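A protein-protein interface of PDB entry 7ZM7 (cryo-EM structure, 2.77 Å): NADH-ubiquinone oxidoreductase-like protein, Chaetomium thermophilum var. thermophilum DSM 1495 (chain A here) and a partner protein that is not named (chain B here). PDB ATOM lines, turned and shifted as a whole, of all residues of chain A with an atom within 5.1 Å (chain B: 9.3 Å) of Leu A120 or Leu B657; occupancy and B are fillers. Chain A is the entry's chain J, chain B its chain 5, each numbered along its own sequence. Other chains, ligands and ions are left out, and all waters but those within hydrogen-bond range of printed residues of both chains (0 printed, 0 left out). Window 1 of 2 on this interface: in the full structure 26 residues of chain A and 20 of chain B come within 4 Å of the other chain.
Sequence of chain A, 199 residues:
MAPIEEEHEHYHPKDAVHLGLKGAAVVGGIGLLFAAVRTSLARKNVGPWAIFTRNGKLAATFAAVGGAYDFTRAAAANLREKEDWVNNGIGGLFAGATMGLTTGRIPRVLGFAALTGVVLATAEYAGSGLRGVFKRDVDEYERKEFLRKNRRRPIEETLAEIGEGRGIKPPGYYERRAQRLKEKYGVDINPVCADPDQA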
ATOM      1  N   VAL A  65      25.879   8.368  30.002  1.00  0.00           N
ATOM      2  CA  VAL A  65      24.888   7.389  29.584  1.00  0.00           C
ATOM      3  C   VAL A  65      23.634   8.080  29.075  1.00  0.00           C
ATOM      4  O   VAL A  65      23.030   7.651  28.084  1.00  0.00           O
ATOM      5  CB  VAL A  65      24.579   6.419  30.736  1.00  0.00           C
ATOM      6  CG1 VAL A  65      23.379   5.552  30.394  1.00  0.00           C
ATOM      7  CG2 VAL A  65      25.788   5.556  31.015  1.00  0.00           C
ATOM      8  N   TYR A  69      22.243   7.835  25.033  1.00  0.00           N
ATOM      9  CA  TYR A  69      20.993   7.149  24.747  1.00  0.00           C
ATOM     10  C   TYR A  69      20.055   8.026  23.934  1.00  0.00           C
ATOM     11  O   TYR A  69      19.653   7.661  22.826  1.00  0.00           O
ATOM     12  CB  TYR A  69      20.324   6.709  26.045  1.00  0.00           C
ATOM     13  CG  TYR A  69      18.879   6.336  25.882  1.00  0.00           C
ATOM     14  CD1 TYR A  69      18.493   5.411  24.933  1.00  0.00           C
ATOM     15  CD2 TYR A  69      17.902   6.903  26.680  1.00  0.00           C
ATOM     16  CE1 TYR A  69      17.176   5.064  24.776  1.00  0.00           C
ATOM     17  CE2 TYR A  69      16.583   6.561  26.535  1.00  0.00           C
ATOM     18  CZ  TYR A  69      16.225   5.633  25.583  1.00  0.00           C
ATOM     19  OH  TYR A  69      14.908   5.282  25.425  1.00  0.00           O
ATOM     20  N   TRP A  85       9.549   0.591  18.155  1.00  0.00           N
ATOM     21  CA  TRP A  85      10.272   0.021  19.281  1.00  0.00           C
ATOM     22  C   TRP A  85      11.745  -0.154  18.995  1.00  0.00           C
ATOM     23  O   TRP A  85      12.529  -0.307  19.935  1.00  0.00           O
ATOM     24  CB  TRP A  85       9.689  -1.336  19.646  1.00  0.00           C
ATOM     25  CG  TRP A  85       9.779  -2.325  18.531  1.00  0.00           C
ATOM     26  CD1 TRP A  85       8.908  -2.473  17.498  1.00  0.00           C
ATOM     27  CD2 TRP A  85      10.808  -3.297  18.330  1.00  0.00           C
ATOM     28  NE1 TRP A  85       9.324  -3.483  16.669  1.00  0.00           N
ATOM     29  CE2 TRP A  85      10.491  -4.004  17.160  1.00  0.00           C
ATOM     30  CE3 TRP A  85      11.967  -3.634  19.026  1.00  0.00           C
ATOM     31  CZ2 TRP A  85      11.287  -5.030  16.671  1.00  0.00           C
ATOM     32  CZ3 TRP A  85      12.756  -4.653  18.542  1.00  0.00           C
ATOM     33  CH2 TRP A  85      12.415  -5.340  17.375  1.00  0.00           C
ATOM     34  N   ASN A  88      14.456   2.575  20.430  1.00  0.00           N
ATOM     35  CA  ASN A  88      14.705   2.396  21.856  1.00  0.00           C
ATOM     36  C   ASN A  88      15.717   1.293  22.113  1.00  0.00           C
ATOM     37  O   ASN A  88      16.392   1.313  23.144  1.00  0.00           O
ATOM     38  CB  ASN A  88      13.408   2.068  22.586  1.00  0.00           C
ATOM     39  CG  ASN A  88      12.643   3.301  23.012  1.00  0.00           C
ATOM     40  OD1 ASN A  88      13.077   4.422  22.783  1.00  0.00           O
ATOM     41  ND2 ASN A  88      11.494   3.097  23.639  1.00  0.00           N
ATOM     42  N   GLY A  89      15.849   0.347  21.194  1.00  0.00           N
ATOM     43  CA  GLY A  89      16.960  -0.574  21.203  1.00  0.00           C
ATOM     44  C   GLY A  89      18.297   0.053  20.869  1.00  0.00           C
ATOM     45  O   GLY A  89      19.238  -0.073  21.656  1.00  0.00           O
ATOM     46  N   GLY A  91      19.460   3.132  20.821  1.00  0.00           N
ATOM     47  CA  GLY A  91      19.916   3.995  21.896  1.00  0.00           C
ATOM     48  C   GLY A  91      20.292   3.217  23.141  1.00  0.00           C
ATOM     49  O   GLY A  91      21.176   3.626  23.897  1.00  0.00           O
ATOM     50  N   GLY A  92      19.617   2.090  23.380  1.00  0.00           N
ATOM     51  CA  GLY A  92      19.958   1.258  24.522  1.00  0.00           C
ATOM     52  C   GLY A  92      21.327   0.611  24.415  1.00  0.00           C
ATOM     53  O   GLY A  92      22.080   0.578  25.389  1.00  0.00           O
ATOM     54  N   ALA A  95      24.011   3.007  24.925  1.00  0.00           N
ATOM     55  CA  ALA A  95      24.062   3.429  26.317  1.00  0.00           C
ATOM     56  C   ALA A  95      24.866   2.446  27.154  1.00  0.00           C
ATOM     57  O   ALA A  95      25.798   2.835  27.866  1.00  0.00           O
ATOM     58  CB  ALA A  95      22.649   3.570  26.869  1.00  0.00           C
ATOM     59  N   MET A  99      28.285   2.585  29.218  1.00  0.00           N
ATOM     60  CA  MET A  99      28.373   2.141  30.606  1.00  0.00           C
ATOM     61  C   MET A  99      29.652   1.354  30.850  1.00  0.00           C
ATOM     62  O   MET A  99      30.348   1.577  31.847  1.00  0.00           O
ATOM     63  CB  MET A  99      27.159   1.286  30.967  1.00  0.00           C
ATOM     64  CG  MET A  99      25.840   2.028  31.000  1.00  0.00           C
ATOM     65  SD  MET A  99      24.474   0.935  31.423  1.00  0.00           S
ATOM     66  CE  MET A  99      23.083   2.048  31.289  1.00  0.00           C
ATOM     67  N   THR A 116      21.599  -3.882  28.581  1.00  0.00           N
ATOM     68  CA  THR A 116      20.900  -2.604  28.531  1.00  0.00           C
ATOM     69  C   THR A 116      19.948  -2.533  27.348  1.00  0.00           C
ATOM     70  O   THR A 116      18.773  -2.206  27.514  1.00  0.00           O
ATOM     71  CB  THR A 116      21.905  -1.456  28.469  1.00  0.00           C
ATOM     72  OG1 THR A 116      22.855  -1.607  29.528  1.00  0.00           O
ATOM     73  CG2 THR A 116      21.197  -0.115  28.612  1.00  0.00           C
ATOM     74  N   GLY A 117      20.430  -2.873  26.156  1.00  0.00           N
ATOM     75  CA  GLY A 117      19.631  -2.674  24.957  1.00  0.00           C
ATOM     76  C   GLY A 117      18.449  -3.617  24.850  1.00  0.00           C
ATOM     77  O   GLY A 117      17.420  -3.272  24.264  1.00  0.00           O
ATOM     78  N   VAL A 118      18.591  -4.832  25.380  1.00  0.00           N
ATOM     79  CA  VAL A 118      17.503  -5.800  25.318  1.00  0.00           C
ATOM     80  C   VAL A 118      16.340  -5.351  26.191  1.00  0.00           C
ATOM     81  O   VAL A 118      15.173  -5.573  25.850  1.00  0.00           O
ATOM     82  CB  VAL A 118      18.012  -7.201  25.702  1.00  0.00           C
ATOM     83  CG1 VAL A 118      16.862  -8.111  26.107  1.00  0.00           C
ATOM     84  CG2 VAL A 118      18.775  -7.810  24.543  1.00  0.00           C
ATOM     85  N   VAL A 119      16.630  -4.714  27.328  1.00  0.00           N
ATOM     86  CA  VAL A 119      15.556  -4.204  28.179  1.00  0.00           C
ATOM     87  C   VAL A 119      14.764  -3.118  27.471  1.00  0.00           C
ATOM     88  O   VAL A 119      13.529  -3.158  27.428  1.00  0.00           O
ATOM     89  CB  VAL A 119      16.116  -3.689  29.508  1.00  0.00           C
ATOM     90  CG1 VAL A 119      15.008  -3.070  30.303  1.00  0.00           C
ATOM     91  CG2 VAL A 119      16.717  -4.831  30.286  1.00  0.00           C
ATOM     92  N   LEU A 120      15.455  -2.136  26.902  1.00  0.00           N
ATOM     93  CA  LEU A 120      14.772  -0.969  26.364  1.00  0.00           C
ATOM     94  C   LEU A 120      13.945  -1.322  25.145  1.00  0.00           C
ATOM     95  O   LEU A 120      12.906  -0.703  24.891  1.00  0.00           O
ATOM     96  CB  LEU A 120      15.781   0.113  26.031  1.00  0.00           C
ATOM     97  CG  LEU A 120      16.089   1.087  27.152  1.00  0.00           C
ATOM     98  CD1 LEU A 120      16.994   0.502  28.203  1.00  0.00           C
ATOM     99  CD2 LEU A 120      16.709   2.276  26.506  1.00  0.00           C
ATOM    100  N   ALA A 121      14.414  -2.275  24.347  1.00  0.00           N
ATOM    101  CA  ALA A 121      13.600  -2.764  23.245  1.00  0.00           C
ATOM    102  C   ALA A 121      12.397  -3.531  23.764  1.00  0.00           C
ATOM    103  O   ALA A 121      11.289  -3.388  23.241  1.00  0.00           O
ATOM    104  CB  ALA A 121      14.446  -3.640  22.330  1.00  0.00           C
ATOM    105  N   THR A 122      12.603  -4.354  24.796  1.00  0.00           N
ATOM    106  CA  THR A 122      11.525  -5.145  25.378  1.00  0.00           C
ATOM    107  C   THR A 122      10.486  -4.259  26.046  1.00  0.00           C
ATOM    108  O   THR A 122       9.284  -4.536  25.974  1.00  0.00           O
ATOM    109  CB  THR A 122      12.102  -6.133  26.385  1.00  0.00           C
ATOM    110  OG1 THR A 122      13.024  -7.002  25.719  1.00  0.00           O
ATOM    111  CG2 THR A 122      11.015  -6.956  27.029  1.00  0.00           C
ATOM    112  N   ALA A 123      10.931  -3.197  26.714  1.00  0.00           N
ATOM    113  CA  ALA A 123       9.988  -2.276  27.330  1.00  0.00           C
ATOM    114  C   ALA A 123       9.099  -1.630  26.282  1.00  0.00           C
ATOM    115  O   ALA A 123       7.883  -1.526  26.461  1.00  0.00           O
ATOM    116  CB  ALA A 123      10.737  -1.218  28.129  1.00  0.00           C
ATOM    117  N   GLU A 124       9.683  -1.216  25.162  1.00  0.00           N
ATOM    118  CA  GLU A 124       8.910  -0.486  24.170  1.00  0.00           C
ATOM    119  C   GLU A 124       8.009  -1.412  23.364  1.00  0.00           C
ATOM    120  O   GLU A 124       6.836  -1.099  23.126  1.00  0.00           O
ATOM    121  CB  GLU A 124       9.842   0.293  23.254  1.00  0.00           C
ATOM    122  CG  GLU A 124       9.102   1.209  22.318  1.00  0.00           C
ATOM    123  CD  GLU A 124       8.416   2.353  23.042  1.00  0.00           C
ATOM    124  OE1 GLU A 124       7.174   2.445  22.973  1.00  0.00           O
ATOM    125  OE2 GLU A 124       9.120   3.159  23.686  1.00  0.00           O
ATOM    126  N   ASP B 651      10.092  10.392  30.293  1.00  0.00           N
ATOM    127  CA  ASP B 651       9.889   9.150  29.501  1.00  0.00           C
ATOM    128  C   ASP B 651      10.128   7.958  30.424  1.00  0.00           C
ATOM    129  O   ASP B 651      11.080   8.008  31.219  1.00  0.00           O
ATOM    130  CB  ASP B 651      10.861   9.076  28.323  1.00  0.00           C
ATOM    131  CG  ASP B 651      10.420   8.117  27.231  1.00  0.00           C
ATOM    132  OD1 ASP B 651       9.300   7.582  27.339  1.00  0.00           O
ATOM    133  OD2 ASP B 651      11.198   7.918  26.278  1.00  0.00           O
ATOM    134  N   TYR B 652       9.278   6.941  30.331  1.00  0.00           N
ATOM    135  CA  TYR B 652       9.454   5.749  31.148  1.00  0.00           C
ATOM    136  C   TYR B 652      10.825   5.137  30.923  1.00  0.00           C
ATOM    137  O   TYR B 652      11.416   4.571  31.846  1.00  0.00           O
ATOM    138  CB  TYR B 652       8.363   4.727  30.835  1.00  0.00           C
ATOM    139  CG  TYR B 652       8.591   4.024  29.527  1.00  0.00           C
ATOM    140  CD1 TYR B 652       8.239   4.621  28.330  1.00  0.00           C
ATOM    141  CD2 TYR B 652       9.185   2.770  29.488  1.00  0.00           C
ATOM    142  CE1 TYR B 652       8.462   3.985  27.131  1.00  0.00           C
ATOM    143  CE2 TYR B 652       9.412   2.128  28.293  1.00  0.00           C
ATOM    144  CZ  TYR B 652       9.048   2.738  27.120  1.00  0.00           C
ATOM    145  OH  TYR B 652       9.273   2.103  25.932  1.00  0.00           O
ATOM    146  N   SER B 653      11.349   5.253  29.704  1.00  0.00           N
ATOM    147  CA  SER B 653      12.663   4.701  29.410  1.00  0.00           C
ATOM    148  C   SER B 653      13.735   5.388  30.233  1.00  0.00           C
ATOM    149  O   SER B 653      14.676   4.737  30.694  1.00  0.00           O
ATOM    150  CB  SER B 653      12.964   4.825  27.922  1.00  0.00           C
ATOM    151  OG  SER B 653      13.047   6.180  27.530  1.00  0.00           O
ATOM    152  N   TYR B 654      13.597   6.698  30.447  1.00  0.00           N
ATOM    153  CA  TYR B 654      14.545   7.421  31.286  1.00  0.00           C
ATOM    154  C   TYR B 654      14.672   6.796  32.662  1.00  0.00           C
ATOM    155  O   TYR B 654      15.760   6.799  33.237  1.00  0.00           O
ATOM    156  CB  TYR B 654      14.138   8.887  31.413  1.00  0.00           C
ATOM    157  CG  TYR B 654      14.454   9.722  30.209  1.00  0.00           C
ATOM    158  CD1 TYR B 654      15.472   9.361  29.343  1.00  0.00           C
ATOM    159  CD2 TYR B 654      13.765  10.894  29.956  1.00  0.00           C
ATOM    160  CE1 TYR B 654      15.775  10.129  28.246  1.00  0.00           C
ATOM    161  CE2 TYR B 654      14.057  11.668  28.862  1.00  0.00           C
ATOM    162  CZ  TYR B 654      15.063  11.282  28.007  1.00  0.00           C
ATOM    163  OH  TYR B 654      15.361  12.056  26.910  1.00  0.00           O
ATOM    164  N   LEU B 655      13.584   6.246  33.200  1.00  0.00           N
ATOM    165  CA  LEU B 655      13.647   5.622  34.518  1.00  0.00           C
ATOM    166  C   LEU B 655      14.480   4.349  34.482  1.00  0.00           C
ATOM    167  O   LEU B 655      15.394   4.174  35.291  1.00  0.00           O
ATOM    168  CB  LEU B 655      12.234   5.328  35.021  1.00  0.00           C
ATOM    169  CG  LEU B 655      12.116   4.732  36.422  1.00  0.00           C
ATOM    170  CD1 LEU B 655      12.701   5.679  37.461  1.00  0.00           C
ATOM    171  CD2 LEU B 655      10.670   4.407  36.738  1.00  0.00           C
ATOM    172  N   LEU B 656      14.204   3.477  33.513  1.00  0.00           N
ATOM    173  CA  LEU B 656      14.879   2.187  33.444  1.00  0.00           C
ATOM    174  C   LEU B 656      16.381   2.355  33.274  1.00  0.00           C
ATOM    175  O   LEU B 656      17.166   1.634  33.900  1.00  0.00           O
ATOM    176  CB  LEU B 656      14.298   1.359  32.300  1.00  0.00           C
ATOM    177  CG  LEU B 656      12.916   0.737  32.478  1.00  0.00           C
ATOM    178  CD1 LEU B 656      12.353   0.290  31.152  1.00  0.00           C
ATOM    179  CD2 LEU B 656      12.998  -0.426  33.433  1.00  0.00           C
ATOM    180  N   LEU B 657      16.804   3.303  32.431  1.00  0.00           N
ATOM    181  CA  LEU B 657      18.224   3.622  32.351  1.00  0.00           C
ATOM    182  C   LEU B 657      18.807   3.893  33.723  1.00  0.00           C
ATOM    183  O   LEU B 657      19.880   3.384  34.052  1.00  0.00           O
ATOM    184  CB  LEU B 657      18.477   4.824  31.442  1.00  0.00           C
ATOM    185  CG  LEU B 657      18.584   4.635  29.934  1.00  0.00           C
ATOM    186  CD1 LEU B 657      19.785   3.774  29.624  1.00  0.00           C
ATOM    187  CD2 LEU B 657      17.349   4.032  29.357  1.00  0.00           C
ATOM    188  N   ILE B 658      18.130   4.697  34.534  1.00  0.00           N
ATOM    189  CA  ILE B 658      18.622   4.953  35.882  1.00  0.00           C
ATOM    190  C   ILE B 658      18.652   3.666  36.695  1.00  0.00           C
ATOM    191  O   ILE B 658      19.662   3.337  37.317  1.00  0.00           O
ATOM    192  CB  ILE B 658      17.778   6.037  36.572  1.00  0.00           C
ATOM    193  CG1 ILE B 658      17.965   7.374  35.866  1.00  0.00           C
ATOM    194  CG2 ILE B 658      18.152   6.154  38.037  1.00  0.00           C
ATOM    195  CD1 ILE B 658      16.711   8.134  35.726  1.00  0.00           C
ATOM    196  N   ILE B 659      17.560   2.906  36.672  1.00  0.00           N
ATOM    197  CA  ILE B 659      17.477   1.695  37.481  1.00  0.00           C
ATOM    198  C   ILE B 659      18.544   0.698  37.053  1.00  0.00           C
ATOM    199  O   ILE B 659      19.267   0.143  37.883  1.00  0.00           O
ATOM    200  CB  ILE B 659      16.061   1.098  37.394  1.00  0.00           C
ATOM    201  CG1 ILE B 659      15.026   2.141  37.816  1.00  0.00           C
ATOM    202  CG2 ILE B 659      15.941  -0.146  38.238  1.00  0.00           C
ATOM    203  CD1 ILE B 659      13.589   1.710  37.639  1.00  0.00           C
ATOM    204  N   ILE B 660      18.671   0.472  35.744  1.00  0.00           N
ATOM    205  CA  ILE B 660      19.675  -0.461  35.241  1.00  0.00           C
ATOM    206  C   ILE B 660      21.075   0.077  35.479  1.00  0.00           C
ATOM    207  O   ILE B 660      22.002  -0.681  35.773  1.00  0.00           O
ATOM    208  CB  ILE B 660      19.430  -0.766  33.755  1.00  0.00           C
ATOM    209  CG1 ILE B 660      18.097  -1.484  33.574  1.00  0.00           C
ATOM    210  CG2 ILE B 660      20.556  -1.594  33.179  1.00  0.00           C
ATOM    211  CD1 ILE B 660      17.363  -1.078  32.319  1.00  0.00           C
ATOM    212  N   LEU B 661      21.260   1.390  35.354  1.00  0.00           N
ATOM    213  CA  LEU B 661      22.583   1.953  35.595  1.00  0.00           C
ATOM    214  C   LEU B 661      22.964   1.806  37.061  1.00  0.00           C
ATOM    215  O   LEU B 661      24.127   1.545  37.384  1.00  0.00           O
ATOM    216  CB  LEU B 661      22.628   3.422  35.170  1.00  0.00           C
ATOM    217  CG  LEU B 661      23.964   4.176  35.143  1.00  0.00           C
ATOM    218  CD1 LEU B 661      23.892   5.307  34.130  1.00  0.00           C
ATOM    219  CD2 LEU B 661      24.445   4.693  36.476  1.00  0.00           C
ATOM    220  N   LEU B 662      21.991   1.962  37.963  1.00  0.00           N
ATOM    221  CA  LEU B 662      22.257   1.738  39.377  1.00  0.00           C
ATOM    222  C   LEU B 662      22.698   0.306  39.651  1.00  0.00           C
ATOM    223  O   LEU B 662      23.682   0.087  40.367  1.00  0.00           O
ATOM    224  CB  LEU B 662      21.030   2.084  40.210  1.00  0.00           C
ATOM    225  CG  LEU B 662      20.604   3.545  40.148  1.00  0.00           C
ATOM    226  CD1 LEU B 662      19.307   3.762  40.906  1.00  0.00           C
ATOM    227  CD2 LEU B 662      21.706   4.448  40.688  1.00  0.00           C
ATOM    228  N   LEU B 663      22.003  -0.681  39.083  1.00  0.00           N
ATOM    229  CA  LEU B 663      22.342  -2.068  39.386  1.00  0.00           C
ATOM    230  C   LEU B 663      23.786  -2.370  39.014  1.00  0.00           C
ATOM    231  O   LEU B 663      24.474  -3.119  39.716  1.00  0.00           O
ATOM    232  CB  LEU B 663      21.392  -3.029  38.668  1.00  0.00           C
ATOM    233  CG  LEU B 663      20.076  -3.460  39.339  1.00  0.00           C
ATOM    234  CD1 LEU B 663      20.319  -4.167  40.675  1.00  0.00           C
ATOM    235  CD2 LEU B 663      19.074  -2.341  39.507  1.00  0.00           C
ATOM    236  N   LEU B 664      24.274  -1.776  37.928  1.00  0.00           N
ATOM    237  CA  LEU B 664      25.641  -2.037  37.502  1.00  0.00           C
ATOM    238  C   LEU B 664      26.654  -1.463  38.488  1.00  0.00           C
ATOM    239  O   LEU B 664      27.717  -2.053  38.706  1.00  0.00           O
ATOM    240  CB  LEU B 664      25.853  -1.476  36.102  1.00  0.00           C
ATOM    241  CG  LEU B 664      24.929  -2.138  35.080  1.00  0.00           C
ATOM    242  CD1 LEU B 664      25.255  -1.682  33.675  1.00  0.00           C
ATOM    243  CD2 LEU B 664      25.005  -3.654  35.177  1.00  0.00           C
ATOM    244  N   LEU B 665      26.340  -0.317  39.094  1.00  0.00           N
ATOM    245  CA  LEU B 665      27.255   0.285  40.056  1.00  0.00           C
ATOM    246  C   LEU B 665      27.346  -0.537  41.337  1.00  0.00           C
ATOM    247  O   LEU B 665      28.397  -0.557  41.981  1.00  0.00           O
ATOM    248  CB  LEU B 665      26.821   1.712  40.365  1.00  0.00           C
ATOM    249  CG  LEU B 665      26.760   2.679  39.183  1.00  0.00           C
ATOM    250  CD1 LEU B 665      26.372   4.060  39.669  1.00  0.00           C
ATOM    251  CD2 LEU B 665      28.053   2.720  38.402  1.00  0.00           C
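OD1 of Asn A88 sits at hydrogen-bond distance from OH of Tyr A69 (3.3 Å).
SD of Met A99 sits at hydrogen-bond distance from OG1 of Thr A116 (3.6 Å).
The side-chain hydroxyl of Ser B653 is in hydrogen-bond range of the side-chain carboxylate of Asp B651, 2.8 Å away.
Among the printed residues, merely in contact across the chains: Val A65 with Leu B661 (3.6 Å), Tyr A69 with Leu B657 (3.9 Å), Ala A95 with Leu B657 (3.98 Å), Met A99 with Leu B664 (3.5 Å), Val A119 with Ile B660 (3.7 Å), Leu A120 with Leu B657 (3.4 Å), Ala A123 with Tyr B652 (3.6 Å) and Ala A123 with Leu B656 (3.7 Å).
Of the printed residues of chain B, Tyr A69 touches Ser B653 and Leu B657.
Of the printed residues of chain B, Ala A95 touches Leu B657.
Printed residues of chain B within 4 Å of Val A119: Ile B660 (3.7 Å).
Leu A120 touches just one residue of chain B: Leu B657 (3.4 Å).
No residue of chain B comes within 4 Å of Ala A121.
Of the printed residues of chain B, Ala A123 touches Tyr B652 and Leu B656.
Of the printed residues of chain A, Leu B656 touches Ala A123 (3.7 Å).
Of chain A, only Tyr A69 (3.9 Å), Ala A95 (3.98 Å) and Leu A120 (3.4 Å) come within 4 Å of Leu B657.
The nearest residue of chain B that does not touch Leu A120 is Ile B660 (4.4 Å).
The nearest printed residue of chain A that does not touch Leu B657 is Met A99 (4.1 Å).
Of the 15 printed residues of chain B, 7 touch a printed residue of chain A.
Hydrophobic or aromatic side chains of chain B that line the printed part of chain A: Tyr B652, Leu B656, Leu B657, Ile B660, Leu B661 and Leu B664.
Along chain B the printed residues that touch a printed residue of chain A span positions 652 to 664.
Hydrophobic or aromatic side chains of chain A that line the printed part of chain B: Val A65, Tyr A69, Ala A95, Met A99, Val A119, Leu A120 and Ala A123.
Among the printed residues, 11 pairs touch across the chains.
The side-chain hydroxyl of Tyr A69 is in hydrogen-bond range of the side-chain hydroxyl of Ser B653.
OH of Tyr B652 sits at hydrogen-bond distance from ND2 of Asn A88 (3.3 Å).
The side-chain carboxylate of Glu A124 sits at hydrogen-bond distance from the side-chain hydroxyl of Tyr B652.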
